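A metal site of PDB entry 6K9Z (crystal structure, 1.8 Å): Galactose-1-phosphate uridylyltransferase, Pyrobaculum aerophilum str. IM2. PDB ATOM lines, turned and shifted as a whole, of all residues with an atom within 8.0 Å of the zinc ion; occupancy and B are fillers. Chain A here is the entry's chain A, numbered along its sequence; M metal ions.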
ATOM      1  N   TYR A 164      14.466  -7.017  -3.112  1.00  0.00           N
ATOM      2  CA  TYR A 164      13.721  -8.279  -3.383  1.00  0.00           C
ATOM      3  C   TYR A 164      14.306  -8.970  -4.617  1.00  0.00           C
ATOM      4  O   TYR A 164      14.586 -10.219  -4.595  1.00  0.00           O
ATOM      5  CB  TYR A 164      12.233  -7.962  -3.551  1.00  0.00           C
ATOM      6  CG  TYR A 164      11.359  -9.167  -3.714  1.00  0.00           C
ATOM      7  CD1 TYR A 164      10.849  -9.817  -2.612  1.00  0.00           C
ATOM      8  CD2 TYR A 164      11.062  -9.659  -4.972  1.00  0.00           C
ATOM      9  CE1 TYR A 164      10.059 -10.953  -2.756  1.00  0.00           C
ATOM     10  CE2 TYR A 164      10.311 -10.818  -5.128  1.00  0.00           C
ATOM     11  CZ  TYR A 164       9.797 -11.449  -4.015  1.00  0.00           C
ATOM     12  OH  TYR A 164       9.031 -12.577  -4.157  1.00  0.00           O
ATOM     13  N   SER A 169      14.099 -12.016  -1.158  1.00  0.00           N
ATOM     14  CA  SER A 169      13.143 -12.050  -0.012  1.00  0.00           C
ATOM     15  C   SER A 169      12.639 -10.629   0.275  1.00  0.00           C
ATOM     16  O   SER A 169      13.234  -9.656  -0.227  1.00  0.00           O
ATOM     17  CB  SER A 169      13.789 -12.670   1.218  1.00  0.00           C
ATOM     18  OG  SER A 169      14.566 -11.713   1.920  1.00  0.00           O
ATOM     19  N   CYS A 170      11.502 -10.504   1.013  1.00  0.00           N
ATOM     20  CA  CYS A 170      10.991  -9.162   1.401  1.00  0.00           C
ATOM     21  C   CYS A 170      11.855  -8.599   2.557  1.00  0.00           C
ATOM     22  O   CYS A 170      11.949  -9.220   3.639  1.00  0.00           O
ATOM     23  CB  CYS A 170       9.528  -9.265   1.836  1.00  0.00           C
ATOM     24  SG  CYS A 170       8.896  -7.773   2.647  1.00  0.00           S
ATOM     25  N   LEU A 171      12.486  -7.410   2.306  1.00  0.00           N
ATOM     26  CA  LEU A 171      13.363  -6.754   3.316  1.00  0.00           C
ATOM     27  C   LEU A 171      12.558  -6.443   4.585  1.00  0.00           C
ATOM     28  O   LEU A 171      13.081  -6.663   5.683  1.00  0.00           O
ATOM     29  CB  LEU A 171      13.978  -5.459   2.796  1.00  0.00           C
ATOM     30  CG  LEU A 171      14.913  -4.758   3.784  1.00  0.00           C
ATOM     31  CD1 LEU A 171      15.959  -5.694   4.366  1.00  0.00           C
ATOM     32  CD2 LEU A 171      15.566  -3.575   3.097  1.00  0.00           C
ATOM     33  N   HIS A 172      11.307  -6.014   4.414  1.00  0.00           N
ATOM     34  CA  HIS A 172      10.454  -5.680   5.594  1.00  0.00           C
ATOM     35  C   HIS A 172      10.255  -6.943   6.448  1.00  0.00           C
ATOM     36  O   HIS A 172      10.301  -6.843   7.674  1.00  0.00           O
ATOM     37  CB  HIS A 172       9.097  -5.131   5.131  1.00  0.00           C
ATOM     38  CG  HIS A 172       9.186  -3.906   4.289  1.00  0.00           C
ATOM     39  ND1 HIS A 172       9.104  -2.639   4.830  1.00  0.00           N
ATOM     40  CD2 HIS A 172       9.324  -3.747   2.958  1.00  0.00           C
ATOM     41  CE1 HIS A 172       9.197  -1.748   3.869  1.00  0.00           C
ATOM     42  NE2 HIS A 172       9.331  -2.402   2.716  1.00  0.00           N
ATOM     43  N   CYS A 173      10.038  -8.083   5.791  1.00  0.00           N
ATOM     44  CA  CYS A 173       9.830  -9.365   6.522  1.00  0.00           C
ATOM     45  C   CYS A 173      11.101  -9.615   7.394  1.00  0.00           C
ATOM     46  O   CYS A 173      10.996 -10.070   8.589  1.00  0.00           O
ATOM     47  CB  CYS A 173       9.581 -10.513   5.536  1.00  0.00           C
ATOM     48  SG  CYS A 173       7.822 -10.684   5.073  1.00  0.00           S
ATOM     49  N   ARG A 174      12.259  -9.400   6.792  1.00  0.00           N
ATOM     50  CA  ARG A 174      13.583  -9.669   7.461  1.00  0.00           C
ATOM     51  C   ARG A 174      13.709  -8.748   8.674  1.00  0.00           C
ATOM     52  O   ARG A 174      14.099  -9.190   9.732  1.00  0.00           O
ATOM     53  CB  ARG A 174      14.695  -9.501   6.426  1.00  0.00           C
ATOM     54  CG  ARG A 174      14.580 -10.456   5.243  1.00  0.00           C
ATOM     55  CD  ARG A 174      15.012 -11.873   5.585  1.00  0.00           C
ATOM     56  NE  ARG A 174      16.213 -11.879   6.427  1.00  0.00           N
ATOM     57  CZ  ARG A 174      17.439 -11.442   6.083  1.00  0.00           C
ATOM     58  NH1 ARG A 174      17.667 -10.910   4.883  1.00  0.00           N
ATOM     59  NH2 ARG A 174      18.437 -11.517   6.962  1.00  0.00           N
ATOM     60  N   ILE A 175      13.383  -7.470   8.504  1.00  0.00           N
ATOM     61  CA  ILE A 175      13.464  -6.485   9.618  1.00  0.00           C
ATOM     62  C   ILE A 175      12.500  -6.871  10.756  1.00  0.00           C
ATOM     63  O   ILE A 175      12.910  -6.963  11.937  1.00  0.00           O
ATOM     64  CB  ILE A 175      13.255  -5.068   9.075  1.00  0.00           C
ATOM     65  CG1 ILE A 175      14.442  -4.602   8.233  1.00  0.00           C
ATOM     66  CG2 ILE A 175      12.986  -4.125  10.239  1.00  0.00           C
ATOM     67  CD1 ILE A 175      14.238  -3.299   7.478  1.00  0.00           C
ATOM     68  N   VAL A 176      11.249  -7.213  10.388  1.00  0.00           N
ATOM     69  CA  VAL A 176      10.214  -7.531  11.410  1.00  0.00           C
ATOM     70  C   VAL A 176      10.682  -8.758  12.202  1.00  0.00           C
ATOM     71  O   VAL A 176      10.529  -8.734  13.419  1.00  0.00           O
ATOM     72  CB  VAL A 176       8.846  -7.751  10.732  1.00  0.00           C
ATOM     73  CG1 VAL A 176       7.828  -8.328  11.692  1.00  0.00           C
ATOM     74  CG2 VAL A 176       8.344  -6.471  10.084  1.00  0.00           C
ATOM     75  N   TYR A 207       4.065  -3.172  12.180  1.00  0.00           N
ATOM     76  CA  TYR A 207       4.050  -4.079  11.002  1.00  0.00           C
ATOM     77  C   TYR A 207       3.262  -5.334  11.296  1.00  0.00           C
ATOM     78  O   TYR A 207       3.300  -5.860  12.415  1.00  0.00           O
ATOM     79  CB  TYR A 207       5.438  -4.579  10.633  1.00  0.00           C
ATOM     80  CG  TYR A 207       6.259  -3.682   9.753  1.00  0.00           C
ATOM     81  CD1 TYR A 207       7.037  -2.648  10.267  1.00  0.00           C
ATOM     82  CD2 TYR A 207       6.370  -3.953   8.401  1.00  0.00           C
ATOM     83  CE1 TYR A 207       7.848  -1.886   9.439  1.00  0.00           C
ATOM     84  CE2 TYR A 207       7.157  -3.207   7.569  1.00  0.00           C
ATOM     85  CZ  TYR A 207       7.920  -2.182   8.086  1.00  0.00           C
ATOM     86  OH  TYR A 207       8.703  -1.463   7.215  1.00  0.00           O
ATOM     87  N   PRO A 208       2.559  -5.869  10.290  1.00  0.00           N
ATOM     88  CA  PRO A 208       1.944  -7.183  10.444  1.00  0.00           C
ATOM     89  C   PRO A 208       3.050  -8.250  10.363  1.00  0.00           C
ATOM     90  O   PRO A 208       4.033  -8.111   9.601  1.00  0.00           O
ATOM     91  CB  PRO A 208       0.967  -7.236   9.269  1.00  0.00           C
ATOM     92  CG  PRO A 208       1.656  -6.425   8.175  1.00  0.00           C
ATOM     93  CD  PRO A 208       2.434  -5.351   8.926  1.00  0.00           C
ATOM     94  N   LYS A 209       2.878  -9.301  11.178  1.00  0.00           N
ATOM     95  CA  LYS A 209       3.863 -10.405  11.222  1.00  0.00           C
ATOM     96  C   LYS A 209       3.742 -11.217   9.918  1.00  0.00           C
ATOM     97  O   LYS A 209       4.738 -11.789   9.524  1.00  0.00           O
ATOM     98  CB  LYS A 209       3.599 -11.249  12.466  1.00  0.00           C
ATOM     99  CG  LYS A 209       4.108 -10.583  13.741  1.00  0.00           C
ATOM    100  CD  LYS A 209       3.667 -11.297  15.017  1.00  0.00           C
ATOM    101  CE  LYS A 209       4.434 -10.818  16.228  1.00  0.00           C
ATOM    102  NZ  LYS A 209       4.207 -11.711  17.401  1.00  0.00           N
ATOM    103  N   ARG A 210       2.532 -11.337   9.376  1.00  0.00           N
ATOM    104  CA  ARG A 210       2.316 -11.954   8.050  1.00  0.00           C
ATOM    105  C   ARG A 210       2.594 -10.895   6.994  1.00  0.00           C
ATOM    106  O   ARG A 210       2.280  -9.737   7.246  1.00  0.00           O
ATOM    107  CB  ARG A 210       0.930 -12.586   7.948  1.00  0.00           C
ATOM    108  CG  ARG A 210       0.880 -13.970   8.589  1.00  0.00           C
ATOM    109  CD  ARG A 210      -0.475 -14.596   8.365  1.00  0.00           C
ATOM    110  NE  ARG A 210      -1.327 -13.972   9.359  1.00  0.00           N
ATOM    111  CZ  ARG A 210      -2.558 -14.357   9.688  1.00  0.00           C
ATOM    112  NH1 ARG A 210      -3.203 -13.695  10.648  1.00  0.00           N
ATOM    113  NH2 ARG A 210      -3.134 -15.376   9.065  1.00  0.00           N
ATOM    114  N   HIS A 211       3.217 -11.300   5.893  1.00  0.00           N
ATOM    115  CA  HIS A 211       3.442 -10.359   4.756  1.00  0.00           C
ATOM    116  C   HIS A 211       2.074  -9.954   4.214  1.00  0.00           C
ATOM    117  O   HIS A 211       1.352 -10.808   3.643  1.00  0.00           O
ATOM    118  CB  HIS A 211       4.314 -10.975   3.656  1.00  0.00           C
ATOM    119  CG  HIS A 211       4.590 -10.012   2.539  1.00  0.00           C
ATOM    120  ND1 HIS A 211       5.720  -9.176   2.517  1.00  0.00           N
ATOM    121  CD2 HIS A 211       3.859  -9.726   1.429  1.00  0.00           C
ATOM    122  CE1 HIS A 211       5.679  -8.476   1.374  1.00  0.00           C
ATOM    123  NE2 HIS A 211       4.543  -8.785   0.700  1.00  0.00           N
ATOM    124  N   ARG A 212       1.716  -8.684   4.415  1.00  0.00           N
ATOM    125  CA  ARG A 212       0.534  -8.062   3.792  1.00  0.00           C
ATOM    126  C   ARG A 212       1.010  -6.762   3.172  1.00  0.00           C
ATOM    127  O   ARG A 212       1.836  -6.090   3.831  1.00  0.00           O
ATOM    128  CB  ARG A 212      -0.481  -7.730   4.869  1.00  0.00           C
ATOM    129  CG  ARG A 212      -0.890  -8.918   5.735  1.00  0.00           C
ATOM    130  CD  ARG A 212      -1.672  -9.911   4.993  1.00  0.00           C
ATOM    131  NE  ARG A 212      -2.326 -10.871   5.895  1.00  0.00           N
ATOM    132  CZ  ARG A 212      -2.840 -12.018   5.499  1.00  0.00           C
ATOM    133  NH1 ARG A 212      -2.703 -12.380   4.233  1.00  0.00           N
ATOM    134  NH2 ARG A 212      -3.429 -12.838   6.337  1.00  0.00           N
ATOM    135  N   SER A 213       0.506  -6.407   2.005  1.00  0.00           N
ATOM    136  CA  SER A 213       0.888  -5.114   1.361  1.00  0.00           C
ATOM    137  C   SER A 213      -0.267  -4.142   1.208  1.00  0.00           C
ATOM    138  O   SER A 213       0.031  -2.933   0.959  1.00  0.00           O
ATOM    139  CB  SER A 213       1.565  -5.383   0.023  1.00  0.00           C
ATOM    140  OG  SER A 213       0.789  -6.230  -0.784  1.00  0.00           O
ATOM    141  N   THR A 260       1.633  -6.686  -3.462  1.00  0.00           N
ATOM    142  CA  THR A 260       3.055  -6.773  -3.865  1.00  0.00           C
ATOM    143  C   THR A 260       3.811  -7.779  -2.995  1.00  0.00           C
ATOM    144  O   THR A 260       3.734  -7.650  -1.812  1.00  0.00           O
ATOM    145  CB  THR A 260       3.778  -5.448  -3.714  1.00  0.00           C
ATOM    146  OG1 THR A 260       3.641  -4.961  -2.375  1.00  0.00           O
ATOM    147  CG2 THR A 260       3.200  -4.407  -4.648  1.00  0.00           C
ATOM    148  N   GLN A 261       4.634  -8.624  -3.607  1.00  0.00           N
ATOM    149  CA  GLN A 261       5.512  -9.581  -2.896  1.00  0.00           C
ATOM    150  C   GLN A 261       6.649  -8.819  -2.193  1.00  0.00           C
ATOM    151  O   GLN A 261       7.166  -9.351  -1.209  1.00  0.00           O
ATOM    152  CB  GLN A 261       6.071 -10.605  -3.878  1.00  0.00           C
ATOM    153  CG  GLN A 261       5.092 -11.700  -4.224  1.00  0.00           C
ATOM    154  CD  GLN A 261       5.693 -12.644  -5.251  1.00  0.00           C
ATOM    155  OE1 GLN A 261       6.375 -12.230  -6.199  1.00  0.00           O
ATOM    156  NE2 GLN A 261       5.492 -13.941  -5.048  1.00  0.00           N
ATOM    157  N   TYR A 262       7.043  -7.632  -2.677  1.00  0.00           N
ATOM    158  CA  TYR A 262       8.327  -6.978  -2.332  1.00  0.00           C
ATOM    159  C   TYR A 262       8.116  -5.824  -1.353  1.00  0.00           C
ATOM    160  O   TYR A 262       9.113  -5.319  -0.765  1.00  0.00           O
ATOM    161  CB  TYR A 262       9.046  -6.423  -3.563  1.00  0.00           C
ATOM    162  CG  TYR A 262       8.205  -5.517  -4.441  1.00  0.00           C
ATOM    163  CD1 TYR A 262       7.445  -6.053  -5.471  1.00  0.00           C
ATOM    164  CD2 TYR A 262       8.167  -4.145  -4.226  1.00  0.00           C
ATOM    165  CE1 TYR A 262       6.666  -5.251  -6.287  1.00  0.00           C
ATOM    166  CE2 TYR A 262       7.360  -3.332  -5.012  1.00  0.00           C
ATOM    167  CZ  TYR A 262       6.628  -3.893  -6.037  1.00  0.00           C
ATOM    168  OH  TYR A 262       5.843  -3.122  -6.833  1.00  0.00           O
ATOM    169  N   TYR A 263       6.858  -5.423  -1.198  1.00  0.00           N
ATOM    170  CA  TYR A 263       6.519  -4.354  -0.230  1.00  0.00           C
ATOM    171  C   TYR A 263       5.521  -4.877   0.790  1.00  0.00           C
ATOM    172  O   TYR A 263       4.779  -5.818   0.548  1.00  0.00           O
ATOM    173  CB  TYR A 263       6.019  -3.108  -0.947  1.00  0.00           C
ATOM    174  CG  TYR A 263       6.029  -1.849  -0.100  1.00  0.00           C
ATOM    175  CD1 TYR A 263       7.220  -1.257   0.281  1.00  0.00           C
ATOM    176  CD2 TYR A 263       4.851  -1.167   0.215  1.00  0.00           C
ATOM    177  CE1 TYR A 263       7.252  -0.047   0.964  1.00  0.00           C
ATOM    178  CE2 TYR A 263       4.876   0.020   0.942  1.00  0.00           C
ATOM    179  CZ  TYR A 263       6.083   0.581   1.308  1.00  0.00           C
ATOM    180  OH  TYR A 263       6.072   1.789   1.964  1.00  0.00           O
ATOM    181  N   HIS A 264       5.694  -4.357   2.006  1.00  0.00           N
ATOM    182  CA  HIS A 264       4.974  -4.781   3.238  1.00  0.00           C
ATOM    183  C   HIS A 264       4.373  -3.543   3.911  1.00  0.00           C
ATOM    184  O   HIS A 264       5.140  -2.610   4.205  1.00  0.00           O
ATOM    185  CB  HIS A 264       6.020  -5.469   4.117  1.00  0.00           C
ATOM    186  CG  HIS A 264       5.522  -6.325   5.237  1.00  0.00           C
ATOM    187  ND1 HIS A 264       6.112  -7.525   5.539  1.00  0.00           N
ATOM    188  CD2 HIS A 264       4.559  -6.126   6.156  1.00  0.00           C
ATOM    189  CE1 HIS A 264       5.513  -8.059   6.586  1.00  0.00           C
ATOM    190  NE2 HIS A 264       4.560  -7.220   6.986  1.00  0.00           N
ATOM    191  N   LEU A 265       3.037  -3.652   4.237  1.00  0.00           N
ATOM    192  CA  LEU A 265       2.421  -2.395   4.712  1.00  0.00           C
ATOM    193  C   LEU A 265       2.898  -2.142   6.129  1.00  0.00           C
ATOM    194  O   LEU A 265       3.261  -3.121   6.892  1.00  0.00           O
ATOM    195  CB  LEU A 265       0.900  -2.460   4.661  1.00  0.00           C
ATOM    196  CG  LEU A 265       0.187  -3.498   5.501  1.00  0.00           C
ATOM    197  CD1 LEU A 265       0.032  -3.131   6.968  1.00  0.00           C
ATOM    198  CD2 LEU A 265      -1.225  -3.742   4.925  1.00  0.00           C
HETATM  199 ZN    ZN M   1       7.206  -8.780   3.910  1.00  0.00          ZN
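Of the 22 residues printed, 4 come within 4 Å of the zinc ion.
The zinc ion is bound by a ring nitrogen (ND1) of His 211, the side-chain sulfur (SG) of Cys 173, a ring nitrogen (ND1) of His 264 and the side-chain sulfur (SG) of Cys 170. The zinc ion has four donor atoms within binding distance.
NE2 of His 211 sits close to O of Tyr 263 (3.0 Å). O of Pro 208 lies within hydrogen-bond range of NE2 of His 264 (2.8 Å). NE2 of His 264 is in hydrogen-bond range of O of Arg 210, 3.4 Å away. The backbone carbonyl oxygen (O) of Gln 261 lies close to a ring nitrogen (NE2) of His 211, at 3.3 Å. The backbone carbonyl oxygen (O) of Thr 260 sits at hydrogen-bond distance from a ring nitrogen (NE2) of His 211, at 2.9 Å. SG of Cys 170 lies close to N of His 172, at 3.5 Å.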
